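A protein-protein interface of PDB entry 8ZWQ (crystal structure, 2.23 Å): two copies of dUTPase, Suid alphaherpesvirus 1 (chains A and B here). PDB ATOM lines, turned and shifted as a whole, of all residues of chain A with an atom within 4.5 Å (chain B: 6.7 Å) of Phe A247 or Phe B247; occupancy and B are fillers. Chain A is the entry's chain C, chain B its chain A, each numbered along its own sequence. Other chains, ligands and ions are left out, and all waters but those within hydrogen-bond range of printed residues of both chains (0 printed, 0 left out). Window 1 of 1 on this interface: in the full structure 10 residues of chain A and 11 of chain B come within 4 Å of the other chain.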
ATOM      1  N   VAL A  28     -17.648  17.620 -34.658  1.00  0.00           N
ATOM      2  CA  VAL A  28     -17.295  16.205 -34.542  1.00  0.00           C
ATOM      3  C   VAL A  28     -18.595  15.432 -34.330  1.00  0.00           C
ATOM      4  O   VAL A  28     -19.229  15.574 -33.284  1.00  0.00           O
ATOM      5  CB  VAL A  28     -16.332  15.945 -33.372  1.00  0.00           C
ATOM      6  CG1 VAL A  28     -16.039  14.455 -33.174  1.00  0.00           C
ATOM      7  CG2 VAL A  28     -15.089  16.723 -33.549  1.00  0.00           C
ATOM      8  N   VAL A  34     -15.021   8.445 -28.189  1.00  0.00           N
ATOM      9  CA  VAL A  34     -13.842   9.231 -28.532  1.00  0.00           C
ATOM     10  C   VAL A  34     -13.350   9.928 -27.281  1.00  0.00           C
ATOM     11  O   VAL A  34     -14.141  10.523 -26.539  1.00  0.00           O
ATOM     12  CB  VAL A  34     -14.139  10.281 -29.615  1.00  0.00           C
ATOM     13  CG1 VAL A  34     -12.896  11.022 -29.912  1.00  0.00           C
ATOM     14  CG2 VAL A  34     -14.734   9.617 -30.851  1.00  0.00           C
ATOM     15  N   VAL A  36     -11.039  12.936 -25.813  1.00  0.00           N
ATOM     16  CA  VAL A  36     -10.377  14.195 -26.104  1.00  0.00           C
ATOM     17  C   VAL A  36      -9.238  14.335 -25.108  1.00  0.00           C
ATOM     18  O   VAL A  36      -9.464  14.309 -23.893  1.00  0.00           O
ATOM     19  CB  VAL A  36     -11.350  15.391 -26.044  1.00  0.00           C
ATOM     20  CG1 VAL A  36     -10.626  16.676 -26.226  1.00  0.00           C
ATOM     21  CG2 VAL A  36     -12.427  15.253 -27.104  1.00  0.00           C
ATOM     22  N   LEU A  41      -7.929  14.240 -30.525  1.00  0.00           N
ATOM     23  CA  LEU A  41      -8.822  13.111 -30.343  1.00  0.00           C
ATOM     24  C   LEU A  41      -8.003  11.831 -30.291  1.00  0.00           C
ATOM     25  O   LEU A  41      -6.989  11.682 -30.988  1.00  0.00           O
ATOM     26  CB  LEU A  41      -9.888  13.030 -31.447  1.00  0.00           C
ATOM     27  CG  LEU A  41     -10.685  14.298 -31.829  1.00  0.00           C
ATOM     28  CD1 LEU A  41     -11.556  14.026 -33.083  1.00  0.00           C
ATOM     29  CD2 LEU A  41     -11.535  14.872 -30.665  1.00  0.00           C
ATOM     30  N   ALA A 244     -11.226  24.267 -30.456  1.00  0.00           N
ATOM     31  CA  ALA A 244     -12.348  23.707 -29.709  1.00  0.00           C
ATOM     32  C   ALA A 244     -13.062  22.640 -30.531  1.00  0.00           C
ATOM     33  O   ALA A 244     -13.196  22.772 -31.750  1.00  0.00           O
ATOM     34  CB  ALA A 244     -13.334  24.819 -29.321  1.00  0.00           C
ATOM     35  N   TRP A 245     -13.521  21.584 -29.866  1.00  0.00           N
ATOM     36  CA  TRP A 245     -14.295  20.531 -30.519  1.00  0.00           C
ATOM     37  C   TRP A 245     -15.748  20.635 -30.069  1.00  0.00           C
ATOM     38  O   TRP A 245     -16.019  20.786 -28.876  1.00  0.00           O
ATOM     39  CB  TRP A 245     -13.757  19.140 -30.192  1.00  0.00           C
ATOM     40  CG  TRP A 245     -12.283  18.952 -30.450  1.00  0.00           C
ATOM     41  CD1 TRP A 245     -11.253  19.272 -29.607  1.00  0.00           C
ATOM     42  CD2 TRP A 245     -11.671  18.371 -31.620  1.00  0.00           C
ATOM     43  NE1 TRP A 245     -10.055  18.941 -30.180  1.00  0.00           N
ATOM     44  CE2 TRP A 245     -10.280  18.384 -31.413  1.00  0.00           C
ATOM     45  CE3 TRP A 245     -12.169  17.861 -32.823  1.00  0.00           C
ATOM     46  CZ2 TRP A 245      -9.373  17.899 -32.369  1.00  0.00           C
ATOM     47  CZ3 TRP A 245     -11.272  17.380 -33.782  1.00  0.00           C
ATOM     48  CH2 TRP A 245      -9.890  17.398 -33.544  1.00  0.00           C
ATOM     49  N   LEU A 246     -16.678  20.594 -31.020  1.00  0.00           N
ATOM     50  CA  LEU A 246     -18.091  20.465 -30.699  1.00  0.00           C
ATOM     51  C   LEU A 246     -18.504  19.035 -31.017  1.00  0.00           C
ATOM     52  O   LEU A 246     -18.347  18.583 -32.149  1.00  0.00           O
ATOM     53  CB  LEU A 246     -18.937  21.472 -31.479  1.00  0.00           C
ATOM     54  CG  LEU A 246     -20.386  21.739 -31.074  1.00  0.00           C
ATOM     55  CD1 LEU A 246     -20.470  22.772 -29.962  1.00  0.00           C
ATOM     56  CD2 LEU A 246     -21.114  22.271 -32.270  1.00  0.00           C
ATOM     57  N   PHE A 247     -18.976  18.310 -30.009  1.00  0.00           N
ATOM     58  CA  PHE A 247     -19.503  16.958 -30.210  1.00  0.00           C
ATOM     59  C   PHE A 247     -21.012  17.073 -30.404  1.00  0.00           C
ATOM     60  O   PHE A 247     -21.763  17.320 -29.452  1.00  0.00           O
ATOM     61  CB  PHE A 247     -19.146  16.046 -29.039  1.00  0.00           C
ATOM     62  CG  PHE A 247     -17.726  15.492 -29.088  1.00  0.00           C
ATOM     63  CD1 PHE A 247     -16.660  16.207 -28.546  1.00  0.00           C
ATOM     64  CD2 PHE A 247     -17.472  14.257 -29.652  1.00  0.00           C
ATOM     65  CE1 PHE A 247     -15.370  15.723 -28.588  1.00  0.00           C
ATOM     66  CE2 PHE A 247     -16.165  13.745 -29.690  1.00  0.00           C
ATOM     67  CZ  PHE A 247     -15.117  14.484 -29.156  1.00  0.00           C
ATOM     68  N   ALA A 248     -21.451  16.917 -31.650  1.00  0.00           N
ATOM     69  CA  ALA A 248     -22.864  16.964 -31.991  1.00  0.00           C
ATOM     70  C   ALA A 248     -23.376  15.588 -32.403  1.00  0.00           C
ATOM     71  O   ALA A 248     -23.552  15.315 -33.596  1.00  0.00           O
ATOM     72  CB  ALA A 248     -23.095  17.970 -33.118  1.00  0.00           C
ATOM     73  N   ILE B  26     -23.360  22.477 -24.050  1.00  0.00           N
ATOM     74  CA  ILE B  26     -22.700  22.488 -22.752  1.00  0.00           C
ATOM     75  C   ILE B  26     -21.222  22.708 -23.013  1.00  0.00           C
ATOM     76  O   ILE B  26     -20.668  22.215 -23.994  1.00  0.00           O
ATOM     77  CB  ILE B  26     -22.959  21.183 -21.957  1.00  0.00           C
ATOM     78  CG1 ILE B  26     -24.460  21.022 -21.685  1.00  0.00           C
ATOM     79  CG2 ILE B  26     -22.121  21.175 -20.654  1.00  0.00           C
ATOM     80  CD1 ILE B  26     -24.922  19.631 -21.484  1.00  0.00           C
ATOM     81  N   LEU B  27     -20.579  23.453 -22.134  1.00  0.00           N
ATOM     82  CA  LEU B  27     -19.198  23.873 -22.316  1.00  0.00           C
ATOM     83  C   LEU B  27     -18.334  23.150 -21.294  1.00  0.00           C
ATOM     84  O   LEU B  27     -18.593  23.246 -20.093  1.00  0.00           O
ATOM     85  CB  LEU B  27     -19.083  25.388 -22.151  1.00  0.00           C
ATOM     86  CG  LEU B  27     -17.661  25.899 -22.033  1.00  0.00           C
ATOM     87  CD1 LEU B  27     -17.026  25.911 -23.422  1.00  0.00           C
ATOM     88  CD2 LEU B  27     -17.627  27.277 -21.388  1.00  0.00           C
ATOM     89  N   VAL B  28     -17.323  22.421 -21.768  1.00  0.00           N
ATOM     90  CA  VAL B  28     -16.451  21.627 -20.908  1.00  0.00           C
ATOM     91  C   VAL B  28     -15.045  22.176 -21.034  1.00  0.00           C
ATOM     92  O   VAL B  28     -14.515  22.287 -22.145  1.00  0.00           O
ATOM     93  CB  VAL B  28     -16.473  20.128 -21.263  1.00  0.00           C
ATOM     94  CG1 VAL B  28     -15.495  19.368 -20.388  1.00  0.00           C
ATOM     95  CG2 VAL B  28     -17.854  19.548 -21.068  1.00  0.00           C
ATOM     96  N   CYS B  29     -14.447  22.533 -19.905  1.00  0.00           N
ATOM     97  CA  CYS B  29     -13.031  22.853 -19.838  1.00  0.00           C
ATOM     98  C   CYS B  29     -12.343  21.727 -19.072  1.00  0.00           C
ATOM     99  O   CYS B  29     -12.545  21.584 -17.860  1.00  0.00           O
ATOM    100  CB  CYS B  29     -12.795  24.207 -19.180  1.00  0.00           C
ATOM    101  SG  CYS B  29     -11.034  24.619 -19.131  1.00  0.00           S
ATOM    102  N   ALA B  30     -11.525  20.936 -19.782  1.00  0.00           N
ATOM    103  CA  ALA B  30     -11.003  19.670 -19.275  1.00  0.00           C
ATOM    104  C   ALA B  30      -9.490  19.735 -19.105  1.00  0.00           C
ATOM    105  O   ALA B  30      -8.757  19.872 -20.088  1.00  0.00           O
ATOM    106  CB  ALA B  30     -11.385  18.530 -20.213  1.00  0.00           C
ATOM    107  N   GLU B  32      -7.870  17.118 -17.923  1.00  0.00           N
ATOM    108  CA  GLU B  32      -7.450  15.724 -18.026  1.00  0.00           C
ATOM    109  C   GLU B  32      -8.178  15.060 -19.190  1.00  0.00           C
ATOM    110  O   GLU B  32      -9.096  15.652 -19.755  1.00  0.00           O
ATOM    111  CB  GLU B  32      -7.734  14.965 -16.721  1.00  0.00           C
ATOM    112  CG  GLU B  32      -6.852  15.336 -15.571  1.00  0.00           C
ATOM    113  CD  GLU B  32      -5.421  14.962 -15.818  1.00  0.00           C
ATOM    114  OE1 GLU B  32      -5.187  13.814 -16.236  1.00  0.00           O
ATOM    115  OE2 GLU B  32      -4.541  15.820 -15.611  1.00  0.00           O
ATOM    116  N   VAL B  34     -10.890  13.213 -21.244  1.00  0.00           N
ATOM    117  CA  VAL B  34     -12.315  12.929 -21.088  1.00  0.00           C
ATOM    118  C   VAL B  34     -12.803  12.152 -22.308  1.00  0.00           C
ATOM    119  O   VAL B  34     -12.451  12.463 -23.451  1.00  0.00           O
ATOM    120  CB  VAL B  34     -13.151  14.223 -20.884  1.00  0.00           C
ATOM    121  CG1 VAL B  34     -14.634  13.912 -20.715  1.00  0.00           C
ATOM    122  CG2 VAL B  34     -12.637  15.011 -19.687  1.00  0.00           C
ATOM    123  N   THR B  35     -13.627  11.151 -22.074  1.00  0.00           N
ATOM    124  CA  THR B  35     -14.125  10.331 -23.157  1.00  0.00           C
ATOM    125  C   THR B  35     -15.569  10.724 -23.435  1.00  0.00           C
ATOM    126  O   THR B  35     -16.380  10.794 -22.511  1.00  0.00           O
ATOM    127  CB  THR B  35     -13.999   8.837 -22.810  1.00  0.00           C
ATOM    128  OG1 THR B  35     -12.620   8.498 -22.618  1.00  0.00           O
ATOM    129  CG2 THR B  35     -14.545   7.980 -23.952  1.00  0.00           C
ATOM    130  N   VAL B  36     -15.887  11.023 -24.693  1.00  0.00           N
ATOM    131  CA  VAL B  36     -17.274  11.231 -25.083  1.00  0.00           C
ATOM    132  C   VAL B  36     -17.849   9.896 -25.544  1.00  0.00           C
ATOM    133  O   VAL B  36     -17.402   9.334 -26.550  1.00  0.00           O
ATOM    134  CB  VAL B  36     -17.394  12.290 -26.184  1.00  0.00           C
ATOM    135  CG1 VAL B  36     -18.860  12.528 -26.491  1.00  0.00           C
ATOM    136  CG2 VAL B  36     -16.688  13.582 -25.759  1.00  0.00           C
ATOM    137  N   LEU B  41     -20.294  11.905 -20.807  1.00  0.00           N
ATOM    138  CA  LEU B  41     -18.861  11.994 -20.589  1.00  0.00           C
ATOM    139  C   LEU B  41     -18.431  10.835 -19.693  1.00  0.00           C
ATOM    140  O   LEU B  41     -19.127  10.487 -18.725  1.00  0.00           O
ATOM    141  CB  LEU B  41     -18.474  13.342 -19.981  1.00  0.00           C
ATOM    142  CG  LEU B  41     -18.957  14.623 -20.690  1.00  0.00           C
ATOM    143  CD1 LEU B  41     -18.417  15.841 -19.942  1.00  0.00           C
ATOM    144  CD2 LEU B  41     -18.560  14.676 -22.179  1.00  0.00           C
ATOM    145  N   LEU B  59     -12.580  17.995 -15.044  1.00  0.00           N
ATOM    146  CA  LEU B  59     -13.314  18.885 -15.934  1.00  0.00           C
ATOM    147  C   LEU B  59     -14.209  19.829 -15.136  1.00  0.00           C
ATOM    148  O   LEU B  59     -14.611  19.552 -13.999  1.00  0.00           O
ATOM    149  CB  LEU B  59     -14.147  18.095 -16.941  1.00  0.00           C
ATOM    150  CG  LEU B  59     -15.218  17.218 -16.272  1.00  0.00           C
ATOM    151  CD1 LEU B  59     -16.618  17.823 -16.410  1.00  0.00           C
ATOM    152  CD2 LEU B  59     -15.190  15.757 -16.754  1.00  0.00           C
ATOM    153  N   ARG B 242     -28.912  13.194 -26.996  1.00  0.00           N
ATOM    154  CA  ARG B 242     -27.529  13.636 -26.945  1.00  0.00           C
ATOM    155  C   ARG B 242     -27.487  15.159 -27.005  1.00  0.00           C
ATOM    156  O   ARG B 242     -28.037  15.748 -27.947  1.00  0.00           O
ATOM    157  CB  ARG B 242     -26.747  13.058 -28.128  1.00  0.00           C
ATOM    158  CG  ARG B 242     -26.067  11.701 -27.935  1.00  0.00           C
ATOM    159  CD  ARG B 242     -24.702  11.734 -28.643  1.00  0.00           C
ATOM    160  NE  ARG B 242     -23.975  12.920 -28.174  1.00  0.00           N
ATOM    161  CZ  ARG B 242     -23.219  13.702 -28.936  1.00  0.00           C
ATOM    162  NH1 ARG B 242     -23.067  13.434 -30.227  1.00  0.00           N
ATOM    163  NH2 ARG B 242     -22.612  14.761 -28.397  1.00  0.00           N
ATOM    164  N   PRO B 243     -26.864  15.832 -26.043  1.00  0.00           N
ATOM    165  CA  PRO B 243     -26.646  17.275 -26.173  1.00  0.00           C
ATOM    166  C   PRO B 243     -25.279  17.562 -26.776  1.00  0.00           C
ATOM    167  O   PRO B 243     -24.454  16.665 -26.934  1.00  0.00           O
ATOM    168  CB  PRO B 243     -26.715  17.756 -24.723  1.00  0.00           C
ATOM    169  CG  PRO B 243     -26.054  16.613 -23.996  1.00  0.00           C
ATOM    170  CD  PRO B 243     -26.368  15.322 -24.750  1.00  0.00           C
ATOM    171  N   ALA B 244     -25.063  18.831 -27.135  1.00  0.00           N
ATOM    172  CA  ALA B 244     -23.788  19.236 -27.708  1.00  0.00           C
ATOM    173  C   ALA B 244     -22.832  19.598 -26.582  1.00  0.00           C
ATOM    174  O   ALA B 244     -23.177  20.371 -25.673  1.00  0.00           O
ATOM    175  CB  ALA B 244     -23.940  20.399 -28.695  1.00  0.00           C
ATOM    176  N   TRP B 245     -21.660  18.971 -26.618  1.00  0.00           N
ATOM    177  CA  TRP B 245     -20.546  19.269 -25.744  1.00  0.00           C
ATOM    178  C   TRP B 245     -19.551  20.106 -26.530  1.00  0.00           C
ATOM    179  O   TRP B 245     -19.279  19.818 -27.704  1.00  0.00           O
ATOM    180  CB  TRP B 245     -19.860  17.988 -25.258  1.00  0.00           C
ATOM    181  CG  TRP B 245     -20.707  17.067 -24.418  1.00  0.00           C
ATOM    182  CD1 TRP B 245     -21.420  15.967 -24.840  1.00  0.00           C
ATOM    183  CD2 TRP B 245     -20.930  17.175 -23.021  1.00  0.00           C
ATOM    184  NE1 TRP B 245     -22.085  15.410 -23.783  1.00  0.00           N
ATOM    185  CE2 TRP B 245     -21.789  16.125 -22.651  1.00  0.00           C
ATOM    186  CE3 TRP B 245     -20.504  18.074 -22.047  1.00  0.00           C
ATOM    187  CZ2 TRP B 245     -22.219  15.943 -21.329  1.00  0.00           C
ATOM    188  CZ3 TRP B 245     -20.933  17.905 -20.740  1.00  0.00           C
ATOM    189  CH2 TRP B 245     -21.775  16.843 -20.391  1.00  0.00           C
ATOM    190  N   LEU B 246     -19.013  21.140 -25.898  1.00  0.00           N
ATOM    191  CA  LEU B 246     -17.980  21.941 -26.541  1.00  0.00           C
ATOM    192  C   LEU B 246     -16.771  21.935 -25.625  1.00  0.00           C
ATOM    193  O   LEU B 246     -16.855  22.397 -24.484  1.00  0.00           O
ATOM    194  CB  LEU B 246     -18.451  23.367 -26.853  1.00  0.00           C
ATOM    195  CG  LEU B 246     -17.371  24.278 -27.475  1.00  0.00           C
ATOM    196  CD1 LEU B 246     -17.130  24.010 -28.975  1.00  0.00           C
ATOM    197  CD2 LEU B 246     -17.712  25.733 -27.239  1.00  0.00           C
ATOM    198  N   PHE B 247     -15.670  21.350 -26.104  1.00  0.00           N
ATOM    199  CA  PHE B 247     -14.397  21.358 -25.392  1.00  0.00           C
ATOM    200  C   PHE B 247     -13.636  22.618 -25.785  1.00  0.00           C
ATOM    201  O   PHE B 247     -13.505  22.916 -26.974  1.00  0.00           O
ATOM    202  CB  PHE B 247     -13.599  20.092 -25.712  1.00  0.00           C
ATOM    203  CG  PHE B 247     -14.159  18.866 -25.056  1.00  0.00           C
ATOM    204  CD1 PHE B 247     -15.182  18.149 -25.656  1.00  0.00           C
ATOM    205  CD2 PHE B 247     -13.698  18.456 -23.821  1.00  0.00           C
ATOM    206  CE1 PHE B 247     -15.723  17.030 -25.036  1.00  0.00           C
ATOM    207  CE2 PHE B 247     -14.227  17.348 -23.197  1.00  0.00           C
ATOM    208  CZ  PHE B 247     -15.242  16.629 -23.809  1.00  0.00           C
ATOM    209  N   ALA B 248     -13.172  23.370 -24.796  1.00  0.00           N
ATOM    210  CA  ALA B 248     -12.567  24.676 -25.066  1.00  0.00           C
ATOM    211  C   ALA B 248     -11.368  24.914 -24.165  1.00  0.00           C
ATOM    212  O   ALA B 248     -10.687  23.962 -23.773  1.00  0.00           O
ATOM    213  CB  ALA B 248     -13.603  25.798 -24.889  1.00  0.00           C
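O of Trp A245 is in hydrogen-bond range of N of Phe B247 (2.9 Å). O of Phe A247 sits at hydrogen-bond distance from NH2 of Arg B242, at 2.9 Å. The backbone carbonyl oxygen (O) of Trp B245 sits at hydrogen-bond distance from the backbone NH (N) of Phe A247 (2.8 Å). The backbone NH (N) of Val B36 sits at hydrogen-bond distance from the backbone carbonyl oxygen (O) of Val A34 (2.6 Å). The backbone carbonyl oxygen (O) of Val B34 sits at hydrogen-bond distance from the backbone NH (N) of Val A36 (2.8 Å).
The backbone NH of Val B28 sits at hydrogen-bond distance from the backbone carbonyl oxygen of Leu B246, 2.8 Å away. The backbone NH of Ala A248 is in hydrogen-bond range of the backbone carbonyl oxygen of Val A28, 3.1 Å away. N of Ile B26 lies within hydrogen-bond range of O of Ala B244, 2.7 Å away. The backbone NH (N) of Val A28 lies within hydrogen-bond range of the backbone carbonyl oxygen (O) of Leu A246, at 2.8 Å. The backbone carbonyl oxygen of Ile B26 lies within hydrogen-bond range of the backbone NH of Leu B246, at 2.7 Å.
O of Val A34 touches CA of Thr B35, 3.4 Å away. Ala A244 touches Leu B246. Trp A245 touches Leu B246. Leu A246 touches Trp B245. Leu A246 touches Leu B246. Val B36 touches Phe A247 (CG2 to CE1, 3.8 Å). Phe A247 touches Pro B243 (O to O, 3.7 Å). O of Phe A247 touches CA of Ala B244, at 3.3 Å. Phe B247 touches Phe A247. NH1 of Arg B242 touches C of Ala A248, at 3.1 Å.
Val A28 touches none of the printed residues of chain B. Of the printed residues of chain B, Leu A246 touches Trp B245 (3.3 Å) and Leu B246 (3.7 Å). Phe A247 touches six residues of chain B. Printed residues of chain B within 4 Å of Ala A248: Arg B242 (3.1 Å). Leu B59 touches none of the printed residues of chain A.
Of the 9 printed residues of chain A, 7 touch a printed residue of chain B. Printed residues of chain B that touch a printed residue of chain A: Val B34, Thr B35, Val B36, Arg B242, Pro B243, Ala B244, Trp B245, Leu B246 and Phe B247. Hydrophobic or aromatic side chains of chain B that line the printed part of chain A: Val B36, Ala B244, Leu B246 and Phe B247. Among the printed residues, 17 pairs touch across the chains. Among the printed residues, no Asp or Glu carboxylate lies within 4 Å of a Lys or Arg side-chain nitrogen of the other chain.
Val A34 touches Val B36, and with the chains exchanged Val A36 touches Val B34. Ala A244 touches Phe B247, and with the chains exchanged Phe A247 touches Ala B244. Trp B245 touches its own counterpart, Trp A245. Phe A247 touches Val B36, but with the chains exchanged Val A36 does not touch Phe B247 (4.3 Å). Positions printed for both chains: 28, 34, 36, 41, 244, 245, 246, 247 and 248. Of the 17 pairs that touch across the chains among the printed residues, 11 have their exchanged pair printed and touching as well.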
